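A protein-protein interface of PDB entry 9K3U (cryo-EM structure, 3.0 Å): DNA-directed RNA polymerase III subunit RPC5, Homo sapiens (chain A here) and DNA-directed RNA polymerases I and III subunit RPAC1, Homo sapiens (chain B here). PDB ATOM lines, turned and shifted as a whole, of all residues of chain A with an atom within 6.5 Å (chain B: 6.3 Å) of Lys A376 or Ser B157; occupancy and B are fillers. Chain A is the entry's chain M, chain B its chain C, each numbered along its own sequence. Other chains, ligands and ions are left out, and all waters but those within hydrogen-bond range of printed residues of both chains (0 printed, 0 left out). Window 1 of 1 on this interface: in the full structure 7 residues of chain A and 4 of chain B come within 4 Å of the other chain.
The side-chain sulfur (SG) of Cys A378 sits at hydrogen-bond distance from the side-chain hydroxyl (OG) of Ser B157 (3.5 Å).
Among the printed residues, merely in contact across the chains: Ser A342 with Ser B157, Val A344 with Ser B157, Val A348 with Asp B155, Thr A375 with Asp B155, Lys A376 with Ser B157, Lys A376 with Asp B158, Lys A376 with Glu B161 and Leu A377 with Asp B155.
The backbone carbonyl oxygen (O) of Val A344 sits at hydrogen-bond distance from the backbone NH (N) of Ser A339 (3.1 Å).
OD2 of Asp A381 sits at hydrogen-bond distance from OG of Ser A342 (3.2 Å).
The backbone carbonyl oxygen of Val A371 sits at hydrogen-bond distance from the side-chain hydroxyl of Thr A375 (2.8 Å).
OE2 of Glu A380 lies within hydrogen-bond range of SG of Cys A378 (3.2 Å).
The side-chain sulfur (SG) of Cys A378 sits close to the side-chain carboxylate (OD2) of Asp A381 (3.3 Å).
N of Glu B161 lies close to OD2 of Asp B158 (3.3 Å).
Of the 8 printed residues of chain B, 4 touch a printed residue of chain A.
Among the printed residues, 9 pairs touch across the chains.
Among the printed residues, no Asp or Glu carboxylate lies within 4 Å of a Lys or Arg side-chain nitrogen of the other chain.
Of the printed residues of chain B, Ser A342 touches Ser B157.
Of the printed residues of chain B, Val A348 touches Asp B155.
Thr A373 touches none of the printed residues of chain B.
Lys A376 touches just these residues of chain B: Ser B157, Asp B158 and Glu B161.
Of the printed residues of chain B, Leu A377 touches Asp B155.
Of the printed residues of chain B, Cys A378 touches Ser B157 (3.5 Å).
Ser B156 touches none of the printed residues of chain A.
Of chain A, only Ser A342, Val A344, Lys A376 and Cys A378 come within 4 Å of Ser B157.
The nearest printed residue of chain B that does not touch Lys A376 is Asp B155 (4.6 Å).
The nearest printed residue of chain B that does not touch Thr A375 is Ser B157 (6.5 Å).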
ATOM      1  N   SER A 339      15.902  16.500 -17.991  1.00  0.00           N
ATOM      2  CA  SER A 339      14.610  16.693 -18.637  1.00  0.00           C
ATOM      3  C   SER A 339      13.576  15.767 -18.012  1.00  0.00           C
ATOM      4  O   SER A 339      13.800  14.549 -17.967  1.00  0.00           O
ATOM      5  CB  SER A 339      14.719  16.426 -20.135  1.00  0.00           C
ATOM      6  OG  SER A 339      13.497  16.705 -20.793  1.00  0.00           O
ATOM      7  N   SER A 342      12.309  13.370 -21.232  1.00  0.00           N
ATOM      8  CA  SER A 342      13.246  12.520 -21.951  1.00  0.00           C
ATOM      9  C   SER A 342      14.459  12.109 -21.132  1.00  0.00           C
ATOM     10  O   SER A 342      15.104  11.112 -21.482  1.00  0.00           O
ATOM     11  CB  SER A 342      13.736  13.220 -23.228  1.00  0.00           C
ATOM     12  OG  SER A 342      14.380  14.444 -22.922  1.00  0.00           O
ATOM     13  N   VAL A 344      17.297  13.799 -20.774  1.00  0.00           N
ATOM     14  CA  VAL A 344      18.555  14.291 -21.333  1.00  0.00           C
ATOM     15  C   VAL A 344      19.204  15.220 -20.314  1.00  0.00           C
ATOM     16  O   VAL A 344      18.505  15.781 -19.457  1.00  0.00           O
ATOM     17  CB  VAL A 344      18.327  15.003 -22.678  1.00  0.00           C
ATOM     18  CG1 VAL A 344      17.757  14.033 -23.706  1.00  0.00           C
ATOM     19  CG2 VAL A 344      17.410  16.211 -22.509  1.00  0.00           C
ATOM     20  N   VAL A 348      22.013  20.169 -22.479  1.00  0.00           N
ATOM     21  CA  VAL A 348      21.332  20.165 -23.768  1.00  0.00           C
ATOM     22  C   VAL A 348      20.067  21.012 -23.704  1.00  0.00           C
ATOM     23  O   VAL A 348      19.744  21.744 -24.649  1.00  0.00           O
ATOM     24  CB  VAL A 348      21.027  18.720 -24.203  1.00  0.00           C
ATOM     25  CG1 VAL A 348      20.207  18.711 -25.484  1.00  0.00           C
ATOM     26  CG2 VAL A 348      22.323  17.932 -24.381  1.00  0.00           C
ATOM     27  N   VAL A 371      12.786  24.675 -35.190  1.00  0.00           N
ATOM     28  CA  VAL A 371      13.508  24.577 -33.924  1.00  0.00           C
ATOM     29  C   VAL A 371      13.802  23.121 -33.592  1.00  0.00           C
ATOM     30  O   VAL A 371      14.911  22.781 -33.159  1.00  0.00           O
ATOM     31  CB  VAL A 371      12.710  25.264 -32.803  1.00  0.00           C
ATOM     32  CG1 VAL A 371      13.377  25.036 -31.451  1.00  0.00           C
ATOM     33  CG2 VAL A 371      12.569  26.750 -33.089  1.00  0.00           C
ATOM     34  N   ALA A 372      12.817  22.239 -33.781  1.00  0.00           N
ATOM     35  CA  ALA A 372      13.028  20.826 -33.488  1.00  0.00           C
ATOM     36  C   ALA A 372      14.069  20.214 -34.412  1.00  0.00           C
ATOM     37  O   ALA A 372      14.973  19.512 -33.947  1.00  0.00           O
ATOM     38  CB  ALA A 372      11.707  20.065 -33.600  1.00  0.00           C
ATOM     39  N   THR A 373      13.970  20.474 -35.716  1.00  0.00           N
ATOM     40  CA  THR A 373      14.924  19.910 -36.663  1.00  0.00           C
ATOM     41  C   THR A 373      16.339  20.407 -36.391  1.00  0.00           C
ATOM     42  O   THR A 373      17.310  19.684 -36.643  1.00  0.00           O
ATOM     43  CB  THR A 373      14.509  20.252 -38.095  1.00  0.00           C
ATOM     44  OG1 THR A 373      13.187  19.754 -38.344  1.00  0.00           O
ATOM     45  CG2 THR A 373      15.476  19.638 -39.098  1.00  0.00           C
ATOM     46  N   VAL A 374      16.477  21.631 -35.882  1.00  0.00           N
ATOM     47  CA  VAL A 374      17.807  22.174 -35.620  1.00  0.00           C
ATOM     48  C   VAL A 374      18.371  21.603 -34.325  1.00  0.00           C
ATOM     49  O   VAL A 374      19.486  21.069 -34.295  1.00  0.00           O
ATOM     50  CB  VAL A 374      17.765  23.713 -35.586  1.00  0.00           C
ATOM     51  CG1 VAL A 374      19.128  24.272 -35.201  1.00  0.00           C
ATOM     52  CG2 VAL A 374      17.316  24.261 -36.933  1.00  0.00           C
ATOM     53  N   THR A 375      17.613  21.703 -33.229  1.00  0.00           N
ATOM     54  CA  THR A 375      18.118  21.283 -31.928  1.00  0.00           C
ATOM     55  C   THR A 375      18.100  19.772 -31.738  1.00  0.00           C
ATOM     56  O   THR A 375      18.624  19.292 -30.726  1.00  0.00           O
ATOM     57  CB  THR A 375      17.307  21.943 -30.812  1.00  0.00           C
ATOM     58  OG1 THR A 375      15.943  21.508 -30.883  1.00  0.00           O
ATOM     59  CG2 THR A 375      17.361  23.460 -30.929  1.00  0.00           C
ATOM     60  N   LYS A 376      17.521  19.015 -32.668  1.00  0.00           N
ATOM     61  CA  LYS A 376      17.434  17.559 -32.564  1.00  0.00           C
ATOM     62  C   LYS A 376      16.762  17.113 -31.270  1.00  0.00           C
ATOM     63  O   LYS A 376      17.012  16.004 -30.788  1.00  0.00           O
ATOM     64  CB  LYS A 376      18.819  16.915 -32.687  1.00  0.00           C
ATOM     65  CG  LYS A 376      19.552  17.242 -33.981  1.00  0.00           C
ATOM     66  CD  LYS A 376      18.804  16.722 -35.201  1.00  0.00           C
ATOM     67  CE  LYS A 376      19.578  16.993 -36.482  1.00  0.00           C
ATOM     68  NZ  LYS A 376      18.852  16.504 -37.688  1.00  0.00           N
ATOM     69  N   LEU A 377      15.913  17.958 -30.695  1.00  0.00           N
ATOM     70  CA  LEU A 377      15.225  17.645 -29.454  1.00  0.00           C
ATOM     71  C   LEU A 377      13.853  17.041 -29.741  1.00  0.00           C
ATOM     72  O   LEU A 377      13.401  16.963 -30.883  1.00  0.00           O
ATOM     73  CB  LEU A 377      15.085  18.899 -28.590  1.00  0.00           C
ATOM     74  CG  LEU A 377      16.397  19.584 -28.200  1.00  0.00           C
ATOM     75  CD1 LEU A 377      16.123  20.836 -27.386  1.00  0.00           C
ATOM     76  CD2 LEU A 377      17.301  18.632 -27.432  1.00  0.00           C
ATOM     77  N   CYS A 378      13.187  16.608 -28.673  1.00  0.00           N
ATOM     78  CA  CYS A 378      11.897  15.957 -28.814  1.00  0.00           C
ATOM     79  C   CYS A 378      10.769  16.991 -28.836  1.00  0.00           C
ATOM     80  O   CYS A 378      10.920  18.145 -28.414  1.00  0.00           O
ATOM     81  CB  CYS A 378      11.677  14.948 -27.686  1.00  0.00           C
ATOM     82  SG  CYS A 378      11.848  15.632 -26.028  1.00  0.00           S
ATOM     83  N   GLU A 380       7.986  17.180 -27.130  1.00  0.00           N
ATOM     84  CA  GLU A 380       7.508  17.659 -25.835  1.00  0.00           C
ATOM     85  C   GLU A 380       8.447  18.710 -25.252  1.00  0.00           C
ATOM     86  O   GLU A 380       7.991  19.719 -24.703  1.00  0.00           O
ATOM     87  CB  GLU A 380       7.334  16.488 -24.862  1.00  0.00           C
ATOM     88  CG  GLU A 380       8.548  15.576 -24.708  1.00  0.00           C
ATOM     89  CD  GLU A 380       8.591  14.458 -25.736  1.00  0.00           C
ATOM     90  OE1 GLU A 380       7.759  14.471 -26.667  1.00  0.00           O
ATOM     91  OE2 GLU A 380       9.460  13.569 -25.612  1.00  0.00           O
ATOM     92  N   ASP A 381       9.761  18.499 -25.368  1.00  0.00           N
ATOM     93  CA  ASP A 381      10.706  19.494 -24.871  1.00  0.00           C
ATOM     94  C   ASP A 381      10.606  20.791 -25.665  1.00  0.00           C
ATOM     95  O   ASP A 381      10.648  21.883 -25.085  1.00  0.00           O
ATOM     96  CB  ASP A 381      12.129  18.942 -24.924  1.00  0.00           C
ATOM     97  CG  ASP A 381      12.404  17.928 -23.827  1.00  0.00           C
ATOM     98  OD1 ASP A 381      11.481  17.640 -23.037  1.00  0.00           O
ATOM     99  OD2 ASP A 381      13.543  17.419 -23.759  1.00  0.00           O
ATOM    100  N   TYR A 434      25.833  23.801 -32.967  1.00  0.00           N
ATOM    101  CA  TYR A 434      24.874  23.204 -33.891  1.00  0.00           C
ATOM    102  C   TYR A 434      25.290  23.325 -35.350  1.00  0.00           C
ATOM    103  O   TYR A 434      24.640  22.723 -36.212  1.00  0.00           O
ATOM    104  CB  TYR A 434      23.498  23.848 -33.700  1.00  0.00           C
ATOM    105  CG  TYR A 434      22.896  23.621 -32.332  1.00  0.00           C
ATOM    106  CD1 TYR A 434      22.152  22.480 -32.061  1.00  0.00           C
ATOM    107  CD2 TYR A 434      23.067  24.548 -31.313  1.00  0.00           C
ATOM    108  CE1 TYR A 434      21.600  22.267 -30.814  1.00  0.00           C
ATOM    109  CE2 TYR A 434      22.518  24.343 -30.061  1.00  0.00           C
ATOM    110  CZ  TYR A 434      21.785  23.202 -29.817  1.00  0.00           C
ATOM    111  OH  TYR A 434      21.235  22.990 -28.575  1.00  0.00           O
ATOM    112  N   ALA B 153      24.051  11.773 -32.584  1.00  0.00           N
ATOM    113  CA  ALA B 153      24.469  12.941 -31.830  1.00  0.00           C
ATOM    114  C   ALA B 153      24.679  12.578 -30.360  1.00  0.00           C
ATOM    115  O   ALA B 153      24.323  11.493 -29.897  1.00  0.00           O
ATOM    116  CB  ALA B 153      23.436  14.059 -31.961  1.00  0.00           C
ATOM    117  N   ASP B 155      23.288  14.098 -27.661  1.00  0.00           N
ATOM    118  CA  ASP B 155      22.000  14.044 -26.975  1.00  0.00           C
ATOM    119  C   ASP B 155      21.065  13.040 -27.643  1.00  0.00           C
ATOM    120  O   ASP B 155      20.600  12.091 -27.003  1.00  0.00           O
ATOM    121  CB  ASP B 155      21.366  15.440 -26.933  1.00  0.00           C
ATOM    122  CG  ASP B 155      21.307  16.101 -28.297  1.00  0.00           C
ATOM    123  OD1 ASP B 155      21.779  15.489 -29.278  1.00  0.00           O
ATOM    124  OD2 ASP B 155      20.786  17.234 -28.389  1.00  0.00           O
ATOM    125  N   SER B 156      20.791  13.232 -28.931  1.00  0.00           N
ATOM    126  CA  SER B 156      19.925  12.341 -29.702  1.00  0.00           C
ATOM    127  C   SER B 156      18.626  12.055 -28.947  1.00  0.00           C
ATOM    128  O   SER B 156      18.227  10.908 -28.741  1.00  0.00           O
ATOM    129  CB  SER B 156      20.659  11.043 -30.045  1.00  0.00           C
ATOM    130  OG  SER B 156      21.846  11.308 -30.773  1.00  0.00           O
ATOM    131  N   SER B 157      17.964  13.138 -28.534  1.00  0.00           N
ATOM    132  CA  SER B 157      16.716  12.995 -27.792  1.00  0.00           C
ATOM    133  C   SER B 157      15.624  12.360 -28.642  1.00  0.00           C
ATOM    134  O   SER B 157      14.675  11.784 -28.101  1.00  0.00           O
ATOM    135  CB  SER B 157      16.256  14.359 -27.275  1.00  0.00           C
ATOM    136  OG  SER B 157      15.048  14.244 -26.543  1.00  0.00           O
ATOM    137  N   ASP B 158      15.737  12.451 -29.964  1.00  0.00           N
ATOM    138  CA  ASP B 158      14.724  11.875 -30.834  1.00  0.00           C
ATOM    139  C   ASP B 158      15.022  10.396 -31.082  1.00  0.00           C
ATOM    140  O   ASP B 158      16.152  10.042 -31.438  1.00  0.00           O
ATOM    141  CB  ASP B 158      14.670  12.626 -32.164  1.00  0.00           C
ATOM    142  CG  ASP B 158      16.009  12.654 -32.871  1.00  0.00           C
ATOM    143  OD1 ASP B 158      17.046  12.741 -32.181  1.00  0.00           O
ATOM    144  OD2 ASP B 158      16.026  12.587 -34.119  1.00  0.00           O
ATOM    145  N   PRO B 159      14.038   9.508 -30.902  1.00  0.00           N
ATOM    146  CA  PRO B 159      14.276   8.092 -31.219  1.00  0.00           C
ATOM    147  C   PRO B 159      14.678   7.854 -32.661  1.00  0.00           C
ATOM    148  O   PRO B 159      15.432   6.910 -32.924  1.00  0.00           O
ATOM    149  CB  PRO B 159      12.930   7.425 -30.900  1.00  0.00           C
ATOM    150  CG  PRO B 159      12.272   8.338 -29.930  1.00  0.00           C
ATOM    151  CD  PRO B 159      12.705   9.721 -30.309  1.00  0.00           C
ATOM    152  N   GLU B 161      16.792   9.375 -34.395  1.00  0.00           N
ATOM    153  CA  GLU B 161      18.247   9.446 -34.472  1.00  0.00           C
ATOM    154  C   GLU B 161      18.916   8.520 -33.466  1.00  0.00           C
ATOM    155  O   GLU B 161      20.040   8.063 -33.703  1.00  0.00           O
ATOM    156  CB  GLU B 161      18.713  10.886 -34.248  1.00  0.00           C
ATOM    157  CG  GLU B 161      20.211  11.089 -34.399  1.00  0.00           C
ATOM    158  CD  GLU B 161      20.632  12.525 -34.160  1.00  0.00           C
ATOM    159  OE1 GLU B 161      19.755  13.355 -33.835  1.00  0.00           O
ATOM    160  OE2 GLU B 161      21.835  12.827 -34.296  1.00  0.00           O
ATOM    161  N   LEU B 162      18.251   8.233 -32.344  1.00  0.00           N
ATOM    162  CA  LEU B 162      18.870   7.398 -31.319  1.00  0.00           C
ATOM    163  C   LEU B 162      18.927   5.938 -31.749  1.00  0.00           C
ATOM    164  O   LEU B 162      19.945   5.264 -31.542  1.00  0.00           O
ATOM    165  CB  LEU B 162      18.112   7.537 -29.999  1.00  0.00           C
ATOM    166  CG  LEU B 162      18.957   7.937 -28.787  1.00  0.00           C
ATOM    167  CD1 LEU B 162      18.078   8.126 -27.561  1.00  0.00           C
ATOM    168  CD2 LEU B 162      20.046   6.910 -28.511  1.00  0.00           C
